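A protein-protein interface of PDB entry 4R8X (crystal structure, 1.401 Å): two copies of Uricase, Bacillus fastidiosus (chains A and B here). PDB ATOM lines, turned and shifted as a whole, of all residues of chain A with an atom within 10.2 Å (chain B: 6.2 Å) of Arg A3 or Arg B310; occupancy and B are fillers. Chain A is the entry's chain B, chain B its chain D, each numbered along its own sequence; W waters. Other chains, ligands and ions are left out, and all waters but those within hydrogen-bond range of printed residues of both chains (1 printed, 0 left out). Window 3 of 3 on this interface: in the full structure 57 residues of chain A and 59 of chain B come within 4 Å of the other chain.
The guanidinium group of Arg A3 is in hydrogen-bond range of the backbone carbonyl oxygen of Ser B302 (2.9 Å). The guanidinium group (NH2) of Arg A3 is in salt-bridge range of the side-chain carboxylate (OD1) of Asp B307 (2.9 Å). OG of Ser B302 lies within hydrogen-bond range of N of Thr A4 (2.9 Å).
N of Leu A55 sits close to SD of Met A5. The backbone carbonyl oxygen (O) of Leu A55 is in hydrogen-bond range of the side-chain hydroxyl (OG1) of Thr A59, 3.4 Å away. The side-chain hydroxyl (OH) of Tyr B249 is in hydrogen-bond range of the side-chain carboxylate (OE2) of Glu B311 (2.6 Å). OG of Ser B302 lies within hydrogen-bond range of NE2 of His B304 (2.8 Å). N of His B304 sits at hydrogen-bond distance from OD2 of Asp B307 (2.9 Å). OD1 of Asp B307 lies within salt-bridge range of NH2 of Arg B310, 2.8 Å away.
Among the printed residues, pairs that only touch across the chains: Arg A3 with Phe B301 (3.7 Å), Arg A3 with His B304 (3.6 Å), Arg A3 with Arg B310 (3.9 Å), Thr A4 with Phe B301 (3.2 Å), Met A5 with Phe B301 (3.9 Å), Phe A58 with Tyr B249 (3.4 Å), Phe A58 with Phe B301 (3.4 Å) and Thr A59 with Tyr B249 (3.6 Å).
Arg A3 touches just these residues of chain B: Phe B301 (3.7 Å), Ser B302 (2.9 Å), His B304 (3.6 Å), Asp B307 (2.9 Å) and Arg B310 (3.9 Å). Arg B310 touches just one residue of chain A: Arg A3 (3.9 Å). No residue of chain A comes within 4 Å of Val B303. Asp B307 touches one residue of chain A. No residue of chain A comes within 4 Å of Ala B309. No residue of chain A comes within 4 Å of Glu B311. No residue of chain A comes within 4 Å of Ala B313. Of the printed residues of chain B, Phe A58 touches Tyr B249 and Phe B301. Of the printed residues of chain A, Phe B301 touches Arg A3 (3.7 Å), Thr A4 (3.2 Å), Met A5 (3.9 Å) and Phe A58 (3.4 Å). Printed residues of chain B within 4 Å of Met A5: Phe B301. Of the printed residues of chain B, Thr A59 touches Tyr B249. The nearest residue of chain A that does not touch Arg B310 is Leu A55 (6.8 Å). The nearest printed residue of chain B that does not touch Thr A59 is Glu B311 (4.4 Å).
Of the 16 printed residues of chain B, 6 touch a printed residue of chain A. Hydrophobic or aromatic side chains of chain A within 4 Å of the printed part of chain B: Met A5 and Phe A58. Among the printed residues, 11 pairs touch across the chains. Among the printed residues, Asp or Glu carboxylates within 4 Å of a Lys or Arg side-chain nitrogen of the other chain: Arg A3 with Asp B307.
No position is printed for both chains.
Water W1 bridges OE2 of Glu B311 (2.6 Å) and O of Thr A59 (2.8 Å).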
ATOM      1  N   GLU A   2     -23.345 -18.857  -0.106  1.00  0.00           N
ATOM      2  CA  GLU A   2     -24.087 -17.620   0.109  1.00  0.00           C
ATOM      3  C   GLU A   2     -24.238 -16.835  -1.194  1.00  0.00           C
ATOM      4  O   GLU A   2     -23.672 -15.755  -1.342  1.00  0.00           O
ATOM      5  CB  GLU A   2     -23.398 -16.767   1.169  1.00  0.00           C
ATOM      6  N   ARG A   3     -25.010 -17.380  -2.135  1.00  0.00           N
ATOM      7  CA  ARG A   3     -25.115 -16.782  -3.467  1.00  0.00           C
ATOM      8  C   ARG A   3     -25.996 -15.539  -3.530  1.00  0.00           C
ATOM      9  O   ARG A   3     -26.917 -15.357  -2.728  1.00  0.00           O
ATOM     10  CB  ARG A   3     -25.608 -17.807  -4.501  1.00  0.00           C
ATOM     11  CG  ARG A   3     -27.114 -17.828  -4.701  1.00  0.00           C
ATOM     12  CD  ARG A   3     -27.524 -18.715  -5.877  1.00  0.00           C
ATOM     13  NE  ARG A   3     -27.246 -20.138  -5.663  1.00  0.00           N
ATOM     14  CZ  ARG A   3     -26.393 -20.857  -6.391  1.00  0.00           C
ATOM     15  NH1 ARG A   3     -25.719 -20.294  -7.391  1.00  0.00           N
ATOM     16  NH2 ARG A   3     -26.216 -22.147  -6.121  1.00  0.00           N
ATOM     17  N   THR A   4     -25.690 -14.690  -4.505  1.00  0.00           N
ATOM     18  CA  THR A   4     -26.511 -13.546  -4.841  1.00  0.00           C
ATOM     19  C   THR A   4     -27.648 -14.052  -5.706  1.00  0.00           C
ATOM     20  O   THR A   4     -27.426 -14.837  -6.624  1.00  0.00           O
ATOM     21  CB  THR A   4     -25.695 -12.521  -5.642  1.00  0.00           C
ATOM     22  OG1 THR A   4     -24.564 -12.091  -4.872  1.00  0.00           O
ATOM     23  CG2 THR A   4     -26.554 -11.317  -6.007  1.00  0.00           C
ATOM     24  N   MET A   5     -28.868 -13.642  -5.393  1.00  0.00           N
ATOM     25  CA  MET A   5     -30.011 -14.085  -6.177  1.00  0.00           C
ATOM     26  C   MET A   5     -31.202 -13.174  -5.971  1.00  0.00           C
ATOM     27  O   MET A   5     -31.797 -13.155  -4.901  1.00  0.00           O
ATOM     28  CB  MET A   5     -30.399 -15.531  -5.833  1.00  0.00           C
ATOM     29  CG  MET A   5     -31.584 -16.028  -6.662  1.00  0.00           C
ATOM     30  SD  MET A   5     -31.877 -17.807  -6.612  1.00  0.00           S
ATOM     31  CE  MET A   5     -32.147 -18.067  -4.856  1.00  0.00           C
ATOM     32  N   PHE A   6     -31.566 -12.436  -7.015  1.00  0.00           N
ATOM     33  CA  PHE A   6     -32.751 -11.594  -6.974  1.00  0.00           C
ATOM     34  C   PHE A   6     -33.146 -11.242  -8.391  1.00  0.00           C
ATOM     35  O   PHE A   6     -32.365 -11.427  -9.317  1.00  0.00           O
ATOM     36  CB  PHE A   6     -32.527 -10.326  -6.135  1.00  0.00           C
ATOM     37  CG  PHE A   6     -31.387  -9.466  -6.601  1.00  0.00           C
ATOM     38  CD1 PHE A   6     -31.543  -8.580  -7.658  1.00  0.00           C
ATOM     39  CD2 PHE A   6     -30.166  -9.518  -5.954  1.00  0.00           C
ATOM     40  CE1 PHE A   6     -30.489  -7.779  -8.076  1.00  0.00           C
ATOM     41  CE2 PHE A   6     -29.110  -8.724  -6.366  1.00  0.00           C
ATOM     42  CZ  PHE A   6     -29.267  -7.850  -7.425  1.00  0.00           C
ATOM     43  N   LYS A  50     -36.771 -11.635  -3.666  1.00  0.00           N
ATOM     44  CA  LYS A  50     -35.763 -12.557  -3.181  1.00  0.00           C
ATOM     45  C   LYS A  50     -36.418 -13.755  -2.512  1.00  0.00           C
ATOM     46  O   LYS A  50     -37.518 -13.664  -1.948  1.00  0.00           O
ATOM     47  CB  LYS A  50     -34.859 -11.872  -2.154  1.00  0.00           C
ATOM     48  CG  LYS A  50     -34.060 -10.711  -2.669  1.00  0.00           C
ATOM     49  CD  LYS A  50     -33.340 -10.006  -1.530  1.00  0.00           C
ATOM     50  CE  LYS A  50     -32.399  -8.946  -2.056  1.00  0.00           C
ATOM     51  NZ  LYS A  50     -31.712  -8.208  -0.949  1.00  0.00           N
ATOM     52  N   GLY A  51     -35.724 -14.878  -2.568  1.00  0.00           N
ATOM     53  CA  GLY A  51     -36.146 -16.059  -1.838  1.00  0.00           C
ATOM     54  C   GLY A  51     -35.486 -17.299  -2.394  1.00  0.00           C
ATOM     55  O   GLY A  51     -35.306 -17.425  -3.602  1.00  0.00           O
ATOM     56  N   GLU A  52     -35.128 -18.216  -1.500  1.00  0.00           N
ATOM     57  CA  GLU A  52     -34.463 -19.458  -1.877  1.00  0.00           C
ATOM     58  C   GLU A  52     -35.242 -20.229  -2.941  1.00  0.00           C
ATOM     59  O   GLU A  52     -34.658 -20.940  -3.753  1.00  0.00           O
ATOM     60  CB  GLU A  52     -34.273 -20.351  -0.646  1.00  0.00           C
ATOM     61  CG  GLU A  52     -33.453 -19.731   0.477  1.00  0.00           C
ATOM     62  CD  GLU A  52     -33.607 -20.474   1.797  1.00  0.00           C
ATOM     63  OE1 GLU A  52     -33.842 -21.701   1.777  1.00  0.00           O
ATOM     64  OE2 GLU A  52     -33.505 -19.827   2.861  1.00  0.00           O
ATOM     65  N   GLN A  53     -36.561 -20.078  -2.944  1.00  0.00           N
ATOM     66  CA  GLN A  53     -37.412 -20.829  -3.866  1.00  0.00           C
ATOM     67  C   GLN A  53     -37.309 -20.351  -5.317  1.00  0.00           C
ATOM     68  O   GLN A  53     -37.874 -20.964  -6.226  1.00  0.00           O
ATOM     69  CB  GLN A  53     -38.867 -20.788  -3.401  1.00  0.00           C
ATOM     70  CG  GLN A  53     -39.118 -21.539  -2.106  1.00  0.00           C
ATOM     71  CD  GLN A  53     -40.593 -21.778  -1.858  1.00  0.00           C
ATOM     72  OE1 GLN A  53     -41.284 -22.368  -2.692  1.00  0.00           O
ATOM     73  NE2 GLN A  53     -41.088 -21.309  -0.717  1.00  0.00           N
ATOM     74  N   LEU A  54     -36.587 -19.260  -5.534  1.00  0.00           N
ATOM     75  CA  LEU A  54     -36.344 -18.767  -6.882  1.00  0.00           C
ATOM     76  C   LEU A  54     -35.198 -19.486  -7.592  1.00  0.00           C
ATOM     77  O   LEU A  54     -34.978 -19.256  -8.779  1.00  0.00           O
ATOM     78  CB  LEU A  54     -36.055 -17.268  -6.850  1.00  0.00           C
ATOM     79  CG  LEU A  54     -37.156 -16.345  -6.332  1.00  0.00           C
ATOM     80  CD1 LEU A  54     -36.637 -14.920  -6.285  1.00  0.00           C
ATOM     81  CD2 LEU A  54     -38.398 -16.442  -7.209  1.00  0.00           C
ATOM     82  N   LEU A  55     -34.478 -20.354  -6.877  1.00  0.00           N
ATOM     83  CA  LEU A  55     -33.273 -20.983  -7.430  1.00  0.00           C
ATOM     84  C   LEU A  55     -33.467 -21.648  -8.798  1.00  0.00           C
ATOM     85  O   LEU A  55     -32.712 -21.376  -9.731  1.00  0.00           O
ATOM     86  CB  LEU A  55     -32.648 -21.966  -6.437  1.00  0.00           C
ATOM     87  CG  LEU A  55     -31.325 -22.587  -6.889  1.00  0.00           C
ATOM     88  CD1 LEU A  55     -30.321 -21.494  -7.282  1.00  0.00           C
ATOM     89  CD2 LEU A  55     -30.749 -23.484  -5.801  1.00  0.00           C
ATOM     90  N   THR A  56     -34.483 -22.495  -8.933  1.00  0.00           N
ATOM     91  CA  THR A  56     -34.650 -23.244 -10.180  1.00  0.00           C
ATOM     92  C   THR A  56     -35.070 -22.390 -11.376  1.00  0.00           C
ATOM     93  O   THR A  56     -34.972 -22.842 -12.521  1.00  0.00           O
ATOM     94  CB  THR A  56     -35.622 -24.438 -10.046  1.00  0.00           C
ATOM     95  OG1 THR A  56     -36.896 -23.979  -9.586  1.00  0.00           O
ATOM     96  CG2 THR A  56     -35.079 -25.475  -9.072  1.00  0.00           C
ATOM     97  N   SER A  57     -35.527 -21.165 -11.122  1.00  0.00           N
ATOM     98  CA  SER A  57     -35.799 -20.245 -12.225  1.00  0.00           C
ATOM     99  C   SER A  57     -34.500 -19.935 -12.965  1.00  0.00           C
ATOM    100  O   SER A  57     -34.509 -19.711 -14.173  1.00  0.00           O
ATOM    101  CB  SER A  57     -36.507 -18.964 -11.763  1.00  0.00           C
ATOM    102  OG  SER A  57     -35.663 -18.132 -10.983  1.00  0.00           O
ATOM    103  N   PHE A  58     -33.382 -19.959 -12.242  1.00  0.00           N
ATOM    104  CA  PHE A  58     -32.075 -19.815 -12.871  1.00  0.00           C
ATOM    105  C   PHE A  58     -31.502 -21.165 -13.300  1.00  0.00           C
ATOM    106  O   PHE A  58     -31.100 -21.342 -14.451  1.00  0.00           O
ATOM    107  CB  PHE A  58     -31.081 -19.134 -11.932  1.00  0.00           C
ATOM    108  CG  PHE A  58     -31.460 -17.734 -11.542  1.00  0.00           C
ATOM    109  CD1 PHE A  58     -32.337 -17.506 -10.497  1.00  0.00           C
ATOM    110  CD2 PHE A  58     -30.902 -16.641 -12.191  1.00  0.00           C
ATOM    111  CE1 PHE A  58     -32.678 -16.221 -10.122  1.00  0.00           C
ATOM    112  CE2 PHE A  58     -31.238 -15.352 -11.820  1.00  0.00           C
ATOM    113  CZ  PHE A  58     -32.123 -15.138 -10.780  1.00  0.00           C
ATOM    114  N   THR A  59     -31.470 -22.120 -12.372  1.00  0.00           N
ATOM    115  CA  THR A  59     -30.738 -23.355 -12.617  1.00  0.00           C
ATOM    116  C   THR A  59     -31.430 -24.271 -13.620  1.00  0.00           C
ATOM    117  O   THR A  59     -30.775 -25.071 -14.274  1.00  0.00           O
ATOM    118  CB  THR A  59     -30.472 -24.135 -11.316  1.00  0.00           C
ATOM    119  OG1 THR A  59     -31.718 -24.524 -10.730  1.00  0.00           O
ATOM    120  CG2 THR A  59     -29.707 -23.271 -10.331  1.00  0.00           C
ATOM    121  N   GLU A  60     -32.748 -24.150 -13.739  1.00  0.00           N
ATOM    122  CA  GLU A  60     -33.513 -25.035 -14.614  1.00  0.00           C
ATOM    123  C   GLU A  60     -34.395 -24.318 -15.639  1.00  0.00           C
ATOM    124  O   GLU A  60     -35.041 -24.964 -16.464  1.00  0.00           O
ATOM    125  CB  GLU A  60     -34.375 -25.999 -13.779  1.00  0.00           C
ATOM    126  CG  GLU A  60     -33.578 -26.918 -12.865  1.00  0.00           C
ATOM    127  CD  GLU A  60     -34.453 -27.752 -11.949  1.00  0.00           C
ATOM    128  OE1 GLU A  60     -35.697 -27.699 -12.090  1.00  0.00           O
ATOM    129  OE2 GLU A  60     -33.892 -28.461 -11.088  1.00  0.00           O
ATOM    130  N   TYR B 249     -27.158 -18.368 -15.953  1.00  0.00           N
ATOM    131  CA  TYR B 249     -26.671 -19.546 -15.252  1.00  0.00           C
ATOM    132  C   TYR B 249     -25.669 -20.289 -16.139  1.00  0.00           C
ATOM    133  O   TYR B 249     -24.566 -20.642 -15.703  1.00  0.00           O
ATOM    134  CB  TYR B 249     -27.830 -20.473 -14.871  1.00  0.00           C
ATOM    135  CG  TYR B 249     -27.420 -21.716 -14.104  1.00  0.00           C
ATOM    136  CD1 TYR B 249     -26.730 -21.621 -12.902  1.00  0.00           C
ATOM    137  CD2 TYR B 249     -27.735 -22.987 -14.580  1.00  0.00           C
ATOM    138  CE1 TYR B 249     -26.366 -22.758 -12.196  1.00  0.00           C
ATOM    139  CE2 TYR B 249     -27.375 -24.125 -13.878  1.00  0.00           C
ATOM    140  CZ  TYR B 249     -26.689 -24.001 -12.690  1.00  0.00           C
ATOM    141  OH  TYR B 249     -26.323 -25.125 -11.983  1.00  0.00           O
ATOM    142  N   PHE B 301     -27.348 -12.370  -9.865  1.00  0.00           N
ATOM    143  CA  PHE B 301     -27.122 -13.792  -9.629  1.00  0.00           C
ATOM    144  C   PHE B 301     -25.643 -14.131  -9.605  1.00  0.00           C
ATOM    145  O   PHE B 301     -24.858 -13.555 -10.354  1.00  0.00           O
ATOM    146  CB  PHE B 301     -27.820 -14.603 -10.731  1.00  0.00           C
ATOM    147  CG  PHE B 301     -27.963 -16.068 -10.420  1.00  0.00           C
ATOM    148  CD1 PHE B 301     -28.846 -16.503  -9.449  1.00  0.00           C
ATOM    149  CD2 PHE B 301     -27.225 -17.012 -11.116  1.00  0.00           C
ATOM    150  CE1 PHE B 301     -28.984 -17.853  -9.166  1.00  0.00           C
ATOM    151  CE2 PHE B 301     -27.363 -18.359 -10.843  1.00  0.00           C
ATOM    152  CZ  PHE B 301     -28.246 -18.782  -9.865  1.00  0.00           C
ATOM    153  N   SER B 302     -25.259 -15.061  -8.742  1.00  0.00           N
ATOM    154  CA  SER B 302     -23.897 -15.580  -8.756  1.00  0.00           C
ATOM    155  C   SER B 302     -23.879 -17.093  -8.963  1.00  0.00           C
ATOM    156  O   SER B 302     -24.735 -17.816  -8.444  1.00  0.00           O
ATOM    157  CB  SER B 302     -23.135 -15.194  -7.484  1.00  0.00           C
ATOM    158  OG  SER B 302     -23.735 -15.746  -6.327  1.00  0.00           O
ATOM    159  N   VAL B 303     -22.896 -17.543  -9.738  1.00  0.00           N
ATOM    160  CA  VAL B 303     -22.680 -18.945 -10.063  1.00  0.00           C
ATOM    161  C   VAL B 303     -21.313 -19.337  -9.490  1.00  0.00           C
ATOM    162  O   VAL B 303     -20.360 -18.555  -9.556  1.00  0.00           O
ATOM    163  CB  VAL B 303     -22.712 -19.167 -11.586  1.00  0.00           C
ATOM    164  CG1 VAL B 303     -22.736 -20.649 -11.921  1.00  0.00           C
ATOM    165  CG2 VAL B 303     -23.928 -18.483 -12.193  1.00  0.00           C
ATOM    166  N   HIS B 304     -21.225 -20.529  -8.905  1.00  0.00           N
ATOM    167  CA  HIS B 304     -20.043 -20.925  -8.146  1.00  0.00           C
ATOM    168  C   HIS B 304     -19.532 -22.267  -8.647  1.00  0.00           C
ATOM    169  O   HIS B 304     -20.276 -23.003  -9.288  1.00  0.00           O
ATOM    170  CB  HIS B 304     -20.406 -20.984  -6.661  1.00  0.00           C
ATOM    171  CG  HIS B 304     -20.984 -19.701  -6.148  1.00  0.00           C
ATOM    172  ND1 HIS B 304     -20.259 -18.816  -5.380  1.00  0.00           N
ATOM    173  CD2 HIS B 304     -22.201 -19.133  -6.329  1.00  0.00           C
ATOM    174  CE1 HIS B 304     -21.011 -17.767  -5.094  1.00  0.00           C
ATOM    175  NE2 HIS B 304     -22.194 -17.935  -5.659  1.00  0.00           N
ATOM    176  N   GLN B 305     -18.269 -22.584  -8.380  1.00  0.00           N
ATOM    177  CA  GLN B 305     -17.711 -23.856  -8.843  1.00  0.00           C
ATOM    178  C   GLN B 305     -18.540 -25.071  -8.408  1.00  0.00           C
ATOM    179  O   GLN B 305     -18.644 -26.049  -9.140  1.00  0.00           O
ATOM    180  CB  GLN B 305     -16.253 -24.023  -8.400  1.00  0.00           C
ATOM    181  CG  GLN B 305     -15.265 -23.107  -9.126  1.00  0.00           C
ATOM    182  CD  GLN B 305     -15.089 -23.448 -10.603  1.00  0.00           C
ATOM    183  OE1 GLN B 305     -15.661 -24.408 -11.105  1.00  0.00           O
ATOM    184  NE2 GLN B 305     -14.289 -22.650 -11.302  1.00  0.00           N
ATOM    185  N   GLU B 306     -19.163 -24.979  -7.238  1.00  0.00           N
ATOM    186  CA  GLU B 306     -20.022 -26.053  -6.749  1.00  0.00           C
ATOM    187  C   GLU B 306     -21.219 -26.286  -7.675  1.00  0.00           C
ATOM    188  O   GLU B 306     -21.699 -27.413  -7.801  1.00  0.00           O
ATOM    189  CB  GLU B 306     -20.487 -25.770  -5.316  1.00  0.00           C
ATOM    190  CG  GLU B 306     -19.377 -25.834  -4.265  1.00  0.00           C
ATOM    191  CD  GLU B 306     -18.476 -24.603  -4.230  1.00  0.00           C
ATOM    192  OE1 GLU B 306     -18.781 -23.592  -4.903  1.00  0.00           O
ATOM    193  OE2 GLU B 306     -17.451 -24.653  -3.515  1.00  0.00           O
ATOM    194  N   ASP B 307     -21.693 -25.224  -8.329  1.00  0.00           N
ATOM    195  CA  ASP B 307     -22.771 -25.358  -9.309  1.00  0.00           C
ATOM    196  C   ASP B 307     -22.308 -26.174 -10.503  1.00  0.00           C
ATOM    197  O   ASP B 307     -23.011 -27.067 -10.970  1.00  0.00           O
ATOM    198  CB  ASP B 307     -23.271 -23.990  -9.778  1.00  0.00           C
ATOM    199  CG  ASP B 307     -23.944 -23.204  -8.672  1.00  0.00           C
ATOM    200  OD1 ASP B 307     -24.753 -23.799  -7.927  1.00  0.00           O
ATOM    201  OD2 ASP B 307     -23.662 -21.996  -8.547  1.00  0.00           O
ATOM    202  N   LEU B 308     -21.117 -25.861 -11.000  1.00  0.00           N
ATOM    203  CA  LEU B 308     -20.572 -26.573 -12.148  1.00  0.00           C
ATOM    204  C   LEU B 308     -20.364 -28.048 -11.810  1.00  0.00           C
ATOM    205  O   LEU B 308     -20.691 -28.929 -12.605  1.00  0.00           O
ATOM    206  CB  LEU B 308     -19.258 -25.936 -12.585  1.00  0.00           C
ATOM    207  CG  LEU B 308     -18.608 -26.573 -13.812  1.00  0.00           C
ATOM    208  CD1 LEU B 308     -19.480 -26.382 -15.054  1.00  0.00           C
ATOM    209  CD2 LEU B 308     -17.226 -25.995 -14.023  1.00  0.00           C
ATOM    210  N   ALA B 309     -19.843 -28.311 -10.617  1.00  0.00           N
ATOM    211  CA  ALA B 309     -19.650 -29.686 -10.180  1.00  0.00           C
ATOM    212  C   ALA B 309     -20.978 -30.444 -10.117  1.00  0.00           C
ATOM    213  O   ALA B 309     -21.058 -31.612 -10.508  1.00  0.00           O
ATOM    214  CB  ALA B 309     -18.936 -29.725  -8.838  1.00  0.00           C
ATOM    215  N   ARG B 310     -22.019 -29.775  -9.629  1.00  0.00           N
ATOM    216  CA  ARG B 310     -23.344 -30.379  -9.578  1.00  0.00           C
ATOM    217  C   ARG B 310     -23.870 -30.704 -10.967  1.00  0.00           C
ATOM    218  O   ARG B 310     -24.438 -31.770 -11.166  1.00  0.00           O
ATOM    219  CB  ARG B 310     -24.332 -29.483  -8.834  1.00  0.00           C
ATOM    220  CG  ARG B 310     -24.291 -29.653  -7.329  1.00  0.00           C
ATOM    221  CD  ARG B 310     -25.399 -28.881  -6.632  1.00  0.00           C
ATOM    222  NE  ARG B 310     -25.131 -27.448  -6.622  1.00  0.00           N
ATOM    223  CZ  ARG B 310     -24.422 -26.824  -5.683  1.00  0.00           C
ATOM    224  NH1 ARG B 310     -23.903 -27.509  -4.673  1.00  0.00           N
ATOM    225  NH2 ARG B 310     -24.225 -25.515  -5.754  1.00  0.00           N
ATOM    226  N   GLU B 311     -23.676 -29.796 -11.920  1.00  0.00           N
ATOM    227  CA  GLU B 311     -24.124 -30.039 -13.289  1.00  0.00           C
ATOM    228  C   GLU B 311     -23.383 -31.221 -13.915  1.00  0.00           C
ATOM    229  O   GLU B 311     -23.994 -32.071 -14.556  1.00  0.00           O
ATOM    230  CB  GLU B 311     -23.985 -28.777 -14.163  1.00  0.00           C
ATOM    231  CG  GLU B 311     -24.894 -27.605 -13.762  1.00  0.00           C
ATOM    232  CD  GLU B 311     -26.372 -27.931 -13.886  1.00  0.00           C
ATOM    233  OE1 GLU B 311     -26.738 -28.760 -14.746  1.00  0.00           O
ATOM    234  OE2 GLU B 311     -27.169 -27.356 -13.118  1.00  0.00           O
ATOM    235  N   LYS B 312     -22.072 -31.288 -13.700  1.00  0.00           N
ATOM    236  CA  LYS B 312     -21.266 -32.376 -14.249  1.00  0.00           C
ATOM    237  C   LYS B 312     -21.566 -33.725 -13.600  1.00  0.00           C
ATOM    238  O   LYS B 312     -21.301 -34.767 -14.193  1.00  0.00           O
ATOM    239  CB  LYS B 312     -19.772 -32.048 -14.160  1.00  0.00           C
ATOM    240  CG  LYS B 312     -19.354 -30.888 -15.066  1.00  0.00           C
ATOM    241  CD  LYS B 312     -17.843 -30.784 -15.220  1.00  0.00           C
ATOM    242  CE  LYS B 312     -17.481 -29.625 -16.147  1.00  0.00           C
ATOM    243  NZ  LYS B 312     -16.041 -29.582 -16.524  1.00  0.00           N
ATOM    244  N   ALA B 313     -22.138 -33.708 -12.400  1.00  0.00           N
ATOM    245  CA  ALA B 313     -22.449 -34.955 -11.693  1.00  0.00           C
ATOM    246  C   ALA B 313     -23.878 -35.418 -11.948  1.00  0.00           C
ATOM    247  O   ALA B 313     -24.282 -36.491 -11.494  1.00  0.00           O
ATOM    248  CB  ALA B 313     -22.217 -34.794 -10.197  1.00  0.00           C
ATOM    249  N   SER B 314     -24.639 -34.606 -12.673  1.00  0.00           N
ATOM    250  CA  SER B 314     -26.066 -34.852 -12.839  1.00  0.00           C
ATOM    251  C   SER B 314     -26.425 -35.499 -14.171  1.00  0.00           C
ATOM    252  O   SER B 314     -26.019 -35.030 -15.233  1.00  0.00           O
ATOM    253  CB  SER B 314     -26.841 -33.546 -12.676  1.00  0.00           C
ATOM    254  OG  SER B 314     -28.178 -33.698 -13.111  1.00  0.00           O
ATOM    255  N   SER B 317     -28.541 -33.038 -16.439  1.00  0.00           N
ATOM    256  CA  SER B 317     -28.006 -31.720 -16.781  1.00  0.00           C
ATOM    257  C   SER B 317     -28.136 -31.399 -18.266  1.00  0.00           C
ATOM    258  O   SER B 317     -27.959 -32.267 -19.119  1.00  0.00           O
ATOM    259  CB  SER B 317     -26.540 -31.593 -16.350  1.00  0.00           C
ATOM    260  OG  SER B 317     -26.007 -30.325 -16.701  1.00  0.00           O
HETATM  261  O   HOH W   1     -29.761 -27.453 -13.282  1.00  0.00           O
